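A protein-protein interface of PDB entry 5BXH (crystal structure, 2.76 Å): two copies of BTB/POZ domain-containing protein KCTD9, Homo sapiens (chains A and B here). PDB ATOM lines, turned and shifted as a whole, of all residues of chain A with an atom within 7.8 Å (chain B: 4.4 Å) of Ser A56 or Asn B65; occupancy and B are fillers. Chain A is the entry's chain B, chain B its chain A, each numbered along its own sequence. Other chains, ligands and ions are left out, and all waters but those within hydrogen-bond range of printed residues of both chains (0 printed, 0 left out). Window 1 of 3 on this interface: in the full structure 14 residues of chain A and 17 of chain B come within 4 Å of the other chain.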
ATOM      1  N   VAL A  10       8.315 -31.569  15.614  1.00  0.00           N
ATOM      2  CA  VAL A  10       8.887 -30.552  14.742  1.00  0.00           C
ATOM      3  C   VAL A  10      10.349 -30.298  15.097  1.00  0.00           C
ATOM      4  O   VAL A  10      10.655 -29.720  16.143  1.00  0.00           O
ATOM      5  CB  VAL A  10       8.103 -29.230  14.822  1.00  0.00           C
ATOM      6  CG1 VAL A  10       8.681 -28.212  13.852  1.00  0.00           C
ATOM      7  CG2 VAL A  10       6.631 -29.469  14.530  1.00  0.00           C
ATOM      8  N   GLY A  11      11.245 -30.758  14.231  1.00  0.00           N
ATOM      9  CA  GLY A  11      12.669 -30.515  14.382  1.00  0.00           C
ATOM     10  C   GLY A  11      13.322 -31.119  15.611  1.00  0.00           C
ATOM     11  O   GLY A  11      14.489 -30.849  15.890  1.00  0.00           O
ATOM     12  N   GLY A  12      12.579 -31.942  16.346  1.00  0.00           N
ATOM     13  CA  GLY A  12      13.084 -32.540  17.568  1.00  0.00           C
ATOM     14  C   GLY A  12      12.289 -32.107  18.786  1.00  0.00           C
ATOM     15  O   GLY A  12      12.482 -32.627  19.886  1.00  0.00           O
ATOM     16  N   ARG A  13      11.386 -31.153  18.585  1.00  0.00           N
ATOM     17  CA  ARG A  13      10.569 -30.637  19.674  1.00  0.00           C
ATOM     18  C   ARG A  13       9.130 -31.114  19.540  1.00  0.00           C
ATOM     19  O   ARG A  13       8.545 -31.052  18.459  1.00  0.00           O
ATOM     20  CB  ARG A  13      10.626 -29.112  19.700  1.00  0.00           C
ATOM     21  CG  ARG A  13       9.959 -28.479  20.899  1.00  0.00           C
ATOM     22  CD  ARG A  13      10.665 -27.188  21.246  1.00  0.00           C
ATOM     23  NE  ARG A  13       9.755 -26.052  21.291  1.00  0.00           N
ATOM     24  CZ  ARG A  13      10.141 -24.790  21.141  1.00  0.00           C
ATOM     25  NH1 ARG A  13      11.418 -24.510  20.923  1.00  0.00           N
ATOM     26  NH2 ARG A  13       9.251 -23.813  21.199  1.00  0.00           N
ATOM     27  N   PHE A  15       5.209 -31.028  20.024  1.00  0.00           N
ATOM     28  CA  PHE A  15       4.019 -30.224  20.258  1.00  0.00           C
ATOM     29  C   PHE A  15       2.812 -31.144  20.383  1.00  0.00           C
ATOM     30  O   PHE A  15       2.761 -32.189  19.747  1.00  0.00           O
ATOM     31  CB  PHE A  15       3.808 -29.215  19.129  1.00  0.00           C
ATOM     32  CG  PHE A  15       4.945 -28.248  18.955  1.00  0.00           C
ATOM     33  CD1 PHE A  15       6.019 -28.560  18.136  1.00  0.00           C
ATOM     34  CD2 PHE A  15       4.939 -27.026  19.608  1.00  0.00           C
ATOM     35  CE1 PHE A  15       7.067 -27.673  17.972  1.00  0.00           C
ATOM     36  CE2 PHE A  15       5.985 -26.134  19.449  1.00  0.00           C
ATOM     37  CZ  PHE A  15       7.050 -26.459  18.629  1.00  0.00           C
ATOM     38  N   ILE A  53       8.077 -33.657  11.386  1.00  0.00           N
ATOM     39  CA  ILE A  53       8.118 -32.483  10.522  1.00  0.00           C
ATOM     40  C   ILE A  53       9.509 -31.853  10.573  1.00  0.00           C
ATOM     41  O   ILE A  53      10.010 -31.519  11.647  1.00  0.00           O
ATOM     42  CB  ILE A  53       7.062 -31.435  10.929  1.00  0.00           C
ATOM     43  CG1 ILE A  53       5.650 -32.011  10.801  1.00  0.00           C
ATOM     44  CG2 ILE A  53       7.203 -30.179  10.083  1.00  0.00           C
ATOM     45  CD1 ILE A  53       4.564 -31.098  11.349  1.00  0.00           C
ATOM     46  N   ASP A  54      10.126 -31.695   9.406  1.00  0.00           N
ATOM     47  CA  ASP A  54      11.497 -31.198   9.311  1.00  0.00           C
ATOM     48  C   ASP A  54      11.541 -29.678   9.145  1.00  0.00           C
ATOM     49  O   ASP A  54      11.963 -29.176   8.104  1.00  0.00           O
ATOM     50  CB  ASP A  54      12.220 -31.886   8.147  1.00  0.00           C
ATOM     51  CG  ASP A  54      13.708 -31.581   8.110  1.00  0.00           C
ATOM     52  OD1 ASP A  54      14.238 -31.041   9.104  1.00  0.00           O
ATOM     53  OD2 ASP A  54      14.350 -31.895   7.084  1.00  0.00           O
ATOM     54  N   ARG A  55      11.097 -28.954  10.172  1.00  0.00           N
ATOM     55  CA  ARG A  55      11.142 -27.491  10.177  1.00  0.00           C
ATOM     56  C   ARG A  55      11.628 -26.967  11.527  1.00  0.00           C
ATOM     57  O   ARG A  55      11.980 -27.746  12.413  1.00  0.00           O
ATOM     58  CB  ARG A  55       9.764 -26.895   9.862  1.00  0.00           C
ATOM     59  CG  ARG A  55       9.111 -27.399   8.582  1.00  0.00           C
ATOM     60  CD  ARG A  55       9.889 -26.995   7.340  1.00  0.00           C
ATOM     61  NE  ARG A  55       9.930 -25.550   7.149  1.00  0.00           N
ATOM     62  CZ  ARG A  55      10.580 -24.951   6.158  1.00  0.00           C
ATOM     63  NH1 ARG A  55      11.244 -25.678   5.270  1.00  0.00           N
ATOM     64  NH2 ARG A  55      10.569 -23.630   6.053  1.00  0.00           N
ATOM     65  N   SER A  56      11.638 -25.647  11.683  1.00  0.00           N
ATOM     66  CA  SER A  56      12.027 -25.027  12.945  1.00  0.00           C
ATOM     67  C   SER A  56      10.852 -24.956  13.910  1.00  0.00           C
ATOM     68  O   SER A  56       9.819 -24.368  13.589  1.00  0.00           O
ATOM     69  CB  SER A  56      12.587 -23.624  12.712  1.00  0.00           C
ATOM     70  OG  SER A  56      12.946 -23.008  13.937  1.00  0.00           O
ATOM     71  N   PRO A  57      11.007 -25.556  15.099  1.00  0.00           N
ATOM     72  CA  PRO A  57       9.965 -25.506  16.129  1.00  0.00           C
ATOM     73  C   PRO A  57       9.865 -24.130  16.778  1.00  0.00           C
ATOM     74  O   PRO A  57       8.789 -23.754  17.243  1.00  0.00           O
ATOM     75  CB  PRO A  57      10.426 -26.554  17.141  1.00  0.00           C
ATOM     76  CG  PRO A  57      11.908 -26.570  17.000  1.00  0.00           C
ATOM     77  CD  PRO A  57      12.174 -26.343  15.535  1.00  0.00           C
ATOM     78  N   GLU A  58      10.974 -23.396  16.809  1.00  0.00           N
ATOM     79  CA  GLU A  58      10.996 -22.069  17.413  1.00  0.00           C
ATOM     80  C   GLU A  58      10.061 -21.130  16.666  1.00  0.00           C
ATOM     81  O   GLU A  58       9.390 -20.292  17.269  1.00  0.00           O
ATOM     82  CB  GLU A  58      12.417 -21.496  17.430  1.00  0.00           C
ATOM     83  CG  GLU A  58      13.378 -22.212  18.369  1.00  0.00           C
ATOM     84  CD  GLU A  58      13.874 -23.531  17.808  1.00  0.00           C
ATOM     85  OE1 GLU A  58      13.862 -23.691  16.569  1.00  0.00           O
ATOM     86  OE2 GLU A  58      14.273 -24.406  18.605  1.00  0.00           O
ATOM     87  N   TYR A  59      10.020 -21.284  15.347  1.00  0.00           N
ATOM     88  CA  TYR A  59       9.150 -20.468  14.512  1.00  0.00           C
ATOM     89  C   TYR A  59       7.857 -21.206  14.179  1.00  0.00           C
ATOM     90  O   TYR A  59       7.057 -20.737  13.374  1.00  0.00           O
ATOM     91  CB  TYR A  59       9.873 -20.053  13.230  1.00  0.00           C
ATOM     92  CG  TYR A  59      11.085 -19.183  13.478  1.00  0.00           C
ATOM     93  CD1 TYR A  59      10.944 -17.836  13.788  1.00  0.00           C
ATOM     94  CD2 TYR A  59      12.370 -19.707  13.404  1.00  0.00           C
ATOM     95  CE1 TYR A  59      12.047 -17.036  14.019  1.00  0.00           C
ATOM     96  CE2 TYR A  59      13.479 -18.913  13.633  1.00  0.00           C
ATOM     97  CZ  TYR A  59      13.310 -17.578  13.940  1.00  0.00           C
ATOM     98  OH  TYR A  59      14.408 -16.782  14.169  1.00  0.00           O
ATOM     99  N   PHE A  60       7.659 -22.362  14.806  1.00  0.00           N
ATOM    100  CA  PHE A  60       6.430 -23.125  14.625  1.00  0.00           C
ATOM    101  C   PHE A  60       5.394 -22.772  15.689  1.00  0.00           C
ATOM    102  O   PHE A  60       4.197 -22.973  15.486  1.00  0.00           O
ATOM    103  CB  PHE A  60       6.714 -24.628  14.650  1.00  0.00           C
ATOM    104  CG  PHE A  60       5.498 -25.478  14.398  1.00  0.00           C
ATOM    105  CD1 PHE A  60       4.984 -25.610  13.118  1.00  0.00           C
ATOM    106  CD2 PHE A  60       4.870 -26.143  15.439  1.00  0.00           C
ATOM    107  CE1 PHE A  60       3.864 -26.390  12.879  1.00  0.00           C
ATOM    108  CE2 PHE A  60       3.750 -26.925  15.207  1.00  0.00           C
ATOM    109  CZ  PHE A  60       3.246 -27.048  13.925  1.00  0.00           C
ATOM    110  N   GLU A  61       5.860 -22.251  16.823  1.00  0.00           N
ATOM    111  CA  GLU A  61       4.966 -21.823  17.900  1.00  0.00           C
ATOM    112  C   GLU A  61       3.891 -20.834  17.420  1.00  0.00           C
ATOM    113  O   GLU A  61       2.698 -21.069  17.648  1.00  0.00           O
ATOM    114  CB  GLU A  61       5.754 -21.189  19.056  1.00  0.00           C
ATOM    115  CG  GLU A  61       6.983 -21.952  19.513  1.00  0.00           C
ATOM    116  CD  GLU A  61       7.726 -21.228  20.626  1.00  0.00           C
ATOM    117  OE1 GLU A  61       7.100 -20.398  21.318  1.00  0.00           O
ATOM    118  OE2 GLU A  61       8.936 -21.484  20.807  1.00  0.00           O
ATOM    119  N   PRO A  62       4.297 -19.730  16.754  1.00  0.00           N
ATOM    120  CA  PRO A  62       3.253 -18.768  16.388  1.00  0.00           C
ATOM    121  C   PRO A  62       2.324 -19.315  15.311  1.00  0.00           C
ATOM    122  O   PRO A  62       1.186 -18.863  15.197  1.00  0.00           O
ATOM    123  CB  PRO A  62       4.046 -17.560  15.866  1.00  0.00           C
ATOM    124  CG  PRO A  62       5.472 -17.804  16.267  1.00  0.00           C
ATOM    125  CD  PRO A  62       5.617 -19.285  16.273  1.00  0.00           C
ATOM    126  N   ILE A  63       2.811 -20.277  14.532  1.00  0.00           N
ATOM    127  CA  ILE A  63       1.991 -20.920  13.513  1.00  0.00           C
ATOM    128  C   ILE A  63       0.858 -21.702  14.169  1.00  0.00           C
ATOM    129  O   ILE A  63      -0.317 -21.498  13.855  1.00  0.00           O
ATOM    130  CB  ILE A  63       2.820 -21.868  12.622  1.00  0.00           C
ATOM    131  CG1 ILE A  63       4.051 -21.150  12.070  1.00  0.00           C
ATOM    132  CG2 ILE A  63       1.969 -22.420  11.491  1.00  0.00           C
ATOM    133  CD1 ILE A  63       3.729 -19.970  11.185  1.00  0.00           C
ATOM    134  N   GLY A  82      11.273 -15.660   9.842  1.00  0.00           N
ATOM    135  CA  GLY A  82      11.215 -17.094  10.062  1.00  0.00           C
ATOM    136  C   GLY A  82       9.783 -17.587  10.107  1.00  0.00           C
ATOM    137  O   GLY A  82       9.436 -18.600   9.488  1.00  0.00           O
ATOM    138  N   GLU A  85       8.489 -17.686   6.722  1.00  0.00           N
ATOM    139  CA  GLU A  85       9.007 -18.845   5.999  1.00  0.00           C
ATOM    140  C   GLU A  85       8.199 -20.095   6.321  1.00  0.00           C
ATOM    141  O   GLU A  85       7.765 -20.823   5.420  1.00  0.00           O
ATOM    142  CB  GLU A  85      10.484 -19.072   6.332  1.00  0.00           C
ATOM    143  CG  GLU A  85      11.104 -20.277   5.636  1.00  0.00           C
ATOM    144  CD  GLU A  85      11.188 -20.109   4.129  1.00  0.00           C
ATOM    145  OE1 GLU A  85      11.523 -18.996   3.668  1.00  0.00           O
ATOM    146  OE2 GLU A  85      10.918 -21.091   3.404  1.00  0.00           O
ATOM    147  N   GLU A  86       7.990 -20.336   7.611  1.00  0.00           N
ATOM    148  CA  GLU A  86       7.240 -21.510   8.036  1.00  0.00           C
ATOM    149  C   GLU A  86       5.788 -21.432   7.560  1.00  0.00           C
ATOM    150  O   GLU A  86       5.229 -22.426   7.091  1.00  0.00           O
ATOM    151  CB  GLU A  86       7.310 -21.667   9.556  1.00  0.00           C
ATOM    152  CG  GLU A  86       8.736 -21.719  10.105  1.00  0.00           C
ATOM    153  CD  GLU A  86       9.591 -22.788   9.441  1.00  0.00           C
ATOM    154  OE1 GLU A  86       9.044 -23.848   9.066  1.00  0.00           O
ATOM    155  OE2 GLU A  86      10.813 -22.570   9.295  1.00  0.00           O
ATOM    156  N   PHE A  90       3.932 -24.272   5.247  1.00  0.00           N
ATOM    157  CA  PHE A  90       2.706 -24.968   5.619  1.00  0.00           C
ATOM    158  C   PHE A  90       1.503 -24.489   4.806  1.00  0.00           C
ATOM    159  O   PHE A  90       0.488 -25.179   4.722  1.00  0.00           O
ATOM    160  CB  PHE A  90       2.438 -24.809   7.114  1.00  0.00           C
ATOM    161  CG  PHE A  90       3.449 -25.498   7.984  1.00  0.00           C
ATOM    162  CD1 PHE A  90       3.582 -26.875   7.954  1.00  0.00           C
ATOM    163  CD2 PHE A  90       4.260 -24.771   8.839  1.00  0.00           C
ATOM    164  CE1 PHE A  90       4.509 -27.514   8.754  1.00  0.00           C
ATOM    165  CE2 PHE A  90       5.189 -25.405   9.643  1.00  0.00           C
ATOM    166  CZ  PHE A  90       5.313 -26.778   9.600  1.00  0.00           C
ATOM    167  N   GLU B  61      20.726 -24.242  15.766  1.00  0.00           N
ATOM    168  CA  GLU B  61      19.402 -24.011  15.187  1.00  0.00           C
ATOM    169  C   GLU B  61      19.463 -23.287  13.831  1.00  0.00           C
ATOM    170  O   GLU B  61      18.889 -23.770  12.851  1.00  0.00           O
ATOM    171  CB  GLU B  61      18.508 -23.213  16.148  1.00  0.00           C
ATOM    172  CG  GLU B  61      18.655 -23.562  17.616  1.00  0.00           C
ATOM    173  CD  GLU B  61      17.790 -22.684  18.507  1.00  0.00           C
ATOM    174  OE1 GLU B  61      16.869 -22.023  17.982  1.00  0.00           O
ATOM    175  OE2 GLU B  61      18.030 -22.653  19.733  1.00  0.00           O
ATOM    176  N   PRO B  62      20.160 -22.130  13.760  1.00  0.00           N
ATOM    177  CA  PRO B  62      20.135 -21.416  12.479  1.00  0.00           C
ATOM    178  C   PRO B  62      20.901 -22.152  11.383  1.00  0.00           C
ATOM    179  O   PRO B  62      20.608 -21.971  10.201  1.00  0.00           O
ATOM    180  CB  PRO B  62      20.809 -20.075  12.805  1.00  0.00           C
ATOM    181  CG  PRO B  62      20.830 -19.990  14.298  1.00  0.00           C
ATOM    182  CD  PRO B  62      20.963 -21.397  14.756  1.00  0.00           C
ATOM    183  N   ILE B  63      21.875 -22.967  11.779  1.00  0.00           N
ATOM    184  CA  ILE B  63      22.624 -23.785  10.833  1.00  0.00           C
ATOM    185  C   ILE B  63      21.693 -24.774  10.147  1.00  0.00           C
ATOM    186  O   ILE B  63      21.630 -24.844   8.915  1.00  0.00           O
ATOM    187  CB  ILE B  63      23.762 -24.562  11.524  1.00  0.00           C
ATOM    188  CG1 ILE B  63      24.646 -23.616  12.341  1.00  0.00           C
ATOM    189  CG2 ILE B  63      24.578 -25.335  10.499  1.00  0.00           C
ATOM    190  CD1 ILE B  63      25.355 -22.570  11.517  1.00  0.00           C
ATOM    191  N   LEU B  64      20.961 -25.529  10.961  1.00  0.00           N
ATOM    192  CA  LEU B  64      20.026 -26.522  10.454  1.00  0.00           C
ATOM    193  C   LEU B  64      18.902 -25.869   9.655  1.00  0.00           C
ATOM    194  O   LEU B  64      18.483 -26.398   8.629  1.00  0.00           O
ATOM    195  CB  LEU B  64      19.449 -27.350  11.605  1.00  0.00           C
ATOM    196  CG  LEU B  64      18.543 -28.517  11.206  1.00  0.00           C
ATOM    197  CD1 LEU B  64      19.223 -29.397  10.169  1.00  0.00           C
ATOM    198  CD2 LEU B  64      18.155 -29.335  12.429  1.00  0.00           C
ATOM    199  N   ASN B  65      18.423 -24.716  10.117  1.00  0.00           N
ATOM    200  CA  ASN B  65      17.390 -23.989   9.384  1.00  0.00           C
ATOM    201  C   ASN B  65      17.889 -23.514   8.019  1.00  0.00           C
ATOM    202  O   ASN B  65      17.149 -23.548   7.033  1.00  0.00           O
ATOM    203  CB  ASN B  65      16.880 -22.806  10.210  1.00  0.00           C
ATOM    204  CG  ASN B  65      16.043 -23.248  11.395  1.00  0.00           C
ATOM    205  OD1 ASN B  65      15.424 -24.312  11.369  1.00  0.00           O
ATOM    206  ND2 ASN B  65      16.023 -22.433  12.446  1.00  0.00           N
ATOM    207  N   TYR B  66      19.148 -23.085   7.961  1.00  0.00           N
ATOM    208  CA  TYR B  66      19.757 -22.700   6.690  1.00  0.00           C
ATOM    209  C   TYR B  66      19.910 -23.921   5.794  1.00  0.00           C
ATOM    210  O   TYR B  66      19.818 -23.818   4.572  1.00  0.00           O
ATOM    211  CB  TYR B  66      21.118 -22.030   6.902  1.00  0.00           C
ATOM    212  CG  TYR B  66      21.811 -21.623   5.613  1.00  0.00           C
ATOM    213  CD1 TYR B  66      21.504 -20.423   4.984  1.00  0.00           C
ATOM    214  CD2 TYR B  66      22.774 -22.439   5.027  1.00  0.00           C
ATOM    215  CE1 TYR B  66      22.134 -20.046   3.807  1.00  0.00           C
ATOM    216  CE2 TYR B  66      23.408 -22.069   3.849  1.00  0.00           C
ATOM    217  CZ  TYR B  66      23.083 -20.873   3.246  1.00  0.00           C
ATOM    218  OH  TYR B  66      23.709 -20.500   2.077  1.00  0.00           O
ATOM    219  N   LEU B  67      20.153 -25.076   6.401  1.00  0.00           N
ATOM    220  CA  LEU B  67      20.189 -26.320   5.643  1.00  0.00           C
ATOM    221  C   LEU B  67      18.802 -26.641   5.096  1.00  0.00           C
ATOM    222  O   LEU B  67      18.667 -27.246   4.033  1.00  0.00           O
ATOM    223  CB  LEU B  67      20.696 -27.475   6.507  1.00  0.00           C
ATOM    224  CG  LEU B  67      22.160 -27.891   6.336  1.00  0.00           C
ATOM    225  CD1 LEU B  67      23.104 -26.768   6.733  1.00  0.00           C
ATOM    226  CD2 LEU B  67      22.449 -29.149   7.138  1.00  0.00           C
ATOM    227  N   ARG B  68      17.773 -26.220   5.827  1.00  0.00           N
ATOM    228  CA  ARG B  68      16.395 -26.531   5.468  1.00  0.00           C
ATOM    229  C   ARG B  68      15.849 -25.641   4.346  1.00  0.00           C
ATOM    230  O   ARG B  68      15.217 -26.139   3.414  1.00  0.00           O
ATOM    231  CB  ARG B  68      15.489 -26.425   6.701  1.00  0.00           C
ATOM    232  CG  ARG B  68      15.693 -27.534   7.733  1.00  0.00           C
ATOM    233  CD  ARG B  68      14.546 -27.579   8.735  1.00  0.00           C
ATOM    234  NE  ARG B  68      14.950 -27.235  10.097  1.00  0.00           N
ATOM    235  CZ  ARG B  68      14.897 -28.072  11.130  1.00  0.00           C
ATOM    236  NH1 ARG B  68      14.455 -29.312  10.965  1.00  0.00           N
ATOM    237  NH2 ARG B  68      15.282 -27.666  12.332  1.00  0.00           N
ATOM    238  N   HIS B  69      16.085 -24.335   4.431  1.00  0.00           N
ATOM    239  CA  HIS B  69      15.502 -23.415   3.455  1.00  0.00           C
ATOM    240  C   HIS B  69      16.469 -22.342   2.958  1.00  0.00           C
ATOM    241  O   HIS B  69      16.041 -21.311   2.439  1.00  0.00           O
ATOM    242  CB  HIS B  69      14.256 -22.749   4.044  1.00  0.00           C
ATOM    243  CG  HIS B  69      14.473 -22.154   5.400  1.00  0.00           C
ATOM    244  ND1 HIS B  69      15.397 -21.160   5.640  1.00  0.00           N
ATOM    245  CD2 HIS B  69      13.883 -22.415   6.592  1.00  0.00           C
ATOM    246  CE1 HIS B  69      15.369 -20.833   6.919  1.00  0.00           C
ATOM    247  NE2 HIS B  69      14.459 -21.580   7.519  1.00  0.00           N
ATOM    248  N   GLY B  70      17.765 -22.590   3.118  1.00  0.00           N
ATOM    249  CA  GLY B  70      18.795 -21.739   2.546  1.00  0.00           C
ATOM    250  C   GLY B  70      18.728 -20.269   2.912  1.00  0.00           C
ATOM    251  O   GLY B  70      19.103 -19.410   2.115  1.00  0.00           O
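The side-chain hydroxyl (OG) of Ser A56 sits at hydrogen-bond distance from the side-chain amide nitrogen (ND2) of Asn B65, at 3.5 Å. The guanidinium group (NH1) of Arg B68 lies within salt-bridge range of the side-chain carboxylate (OD1) of Asp A54. O of Arg A55 sits close to NH1 of Arg B68, 3.3 Å away.
The side-chain amide nitrogen (ND2) of Asn B65 sits at hydrogen-bond distance from the backbone carbonyl oxygen (O) of Glu B61 (3.2 Å). The guanidinium group of Arg B68 lies within hydrogen-bond range of the side-chain amide oxygen of Asn B65 (3.2 Å). O of Asn B65 lies close to ND1 of His B69, at 3.3 Å. OE2 of Glu A85 is in salt-bridge range of NH2 of Arg A55 (3.7 Å). The side-chain carboxylate (OE1) of Glu A86 is in salt-bridge range of the guanidinium group (NE) of Arg A55 (2.7 Å). The side-chain hydroxyl (OG) of Ser A56 lies within hydrogen-bond range of the side-chain carboxylate (OE1) of Glu A58 (2.9 Å).
His B69 touches Arg A55. OE1 of Glu B61 touches CD of Glu A58, at 3.4 Å. Glu A85 touches His B69.
Of the printed residues of chain B, Asp A54 touches Arg B68 (2.5 Å). Of the printed residues of chain B, Arg A55 touches Arg B68 and His B69. Printed residues of chain B within 4 Å of Ser A56: Asn B65 (3.2 Å). Printed residues of chain A within 4 Å of Glu B61: Glu A58 (3.4 Å). Of chain A, only Ser A56 (3.2 Å) comes within 4 Å of Asn B65. Printed residues of chain A within 4 Å of His B69: Arg A55 and Glu A85. The nearest printed residue of chain B that does not touch Ser A56 is Arg B68 (4.001 Å). The nearest residue of chain A that does not touch Asn B65 is Tyr A59 (4.5 Å). The nearest printed residue of chain B that does not touch Glu A58 is Asn B65 (4.8 Å).
Of the 10 printed residues of chain B, 4 touch a printed residue of chain A. Hydrophobic or aromatic side chains of chain B that line the printed part of chain A: His B69. Printed residues of chain A that touch a printed residue of chain B: Asp A54, Arg A55, Ser A56, Glu A58 and Glu A85. Among the printed residues, 6 pairs touch across the chains. Among the printed residues, Asp or Glu carboxylates within 4 Å of a Lys or Arg side-chain nitrogen of the other chain: Asp A54 with Arg B68 (2.5 Å).
Positions printed for both chains: 61, 62 and 63. Of the 6 pairs that touch across the chains among the printed residues, none has its exchanged pair printed and touching as well.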
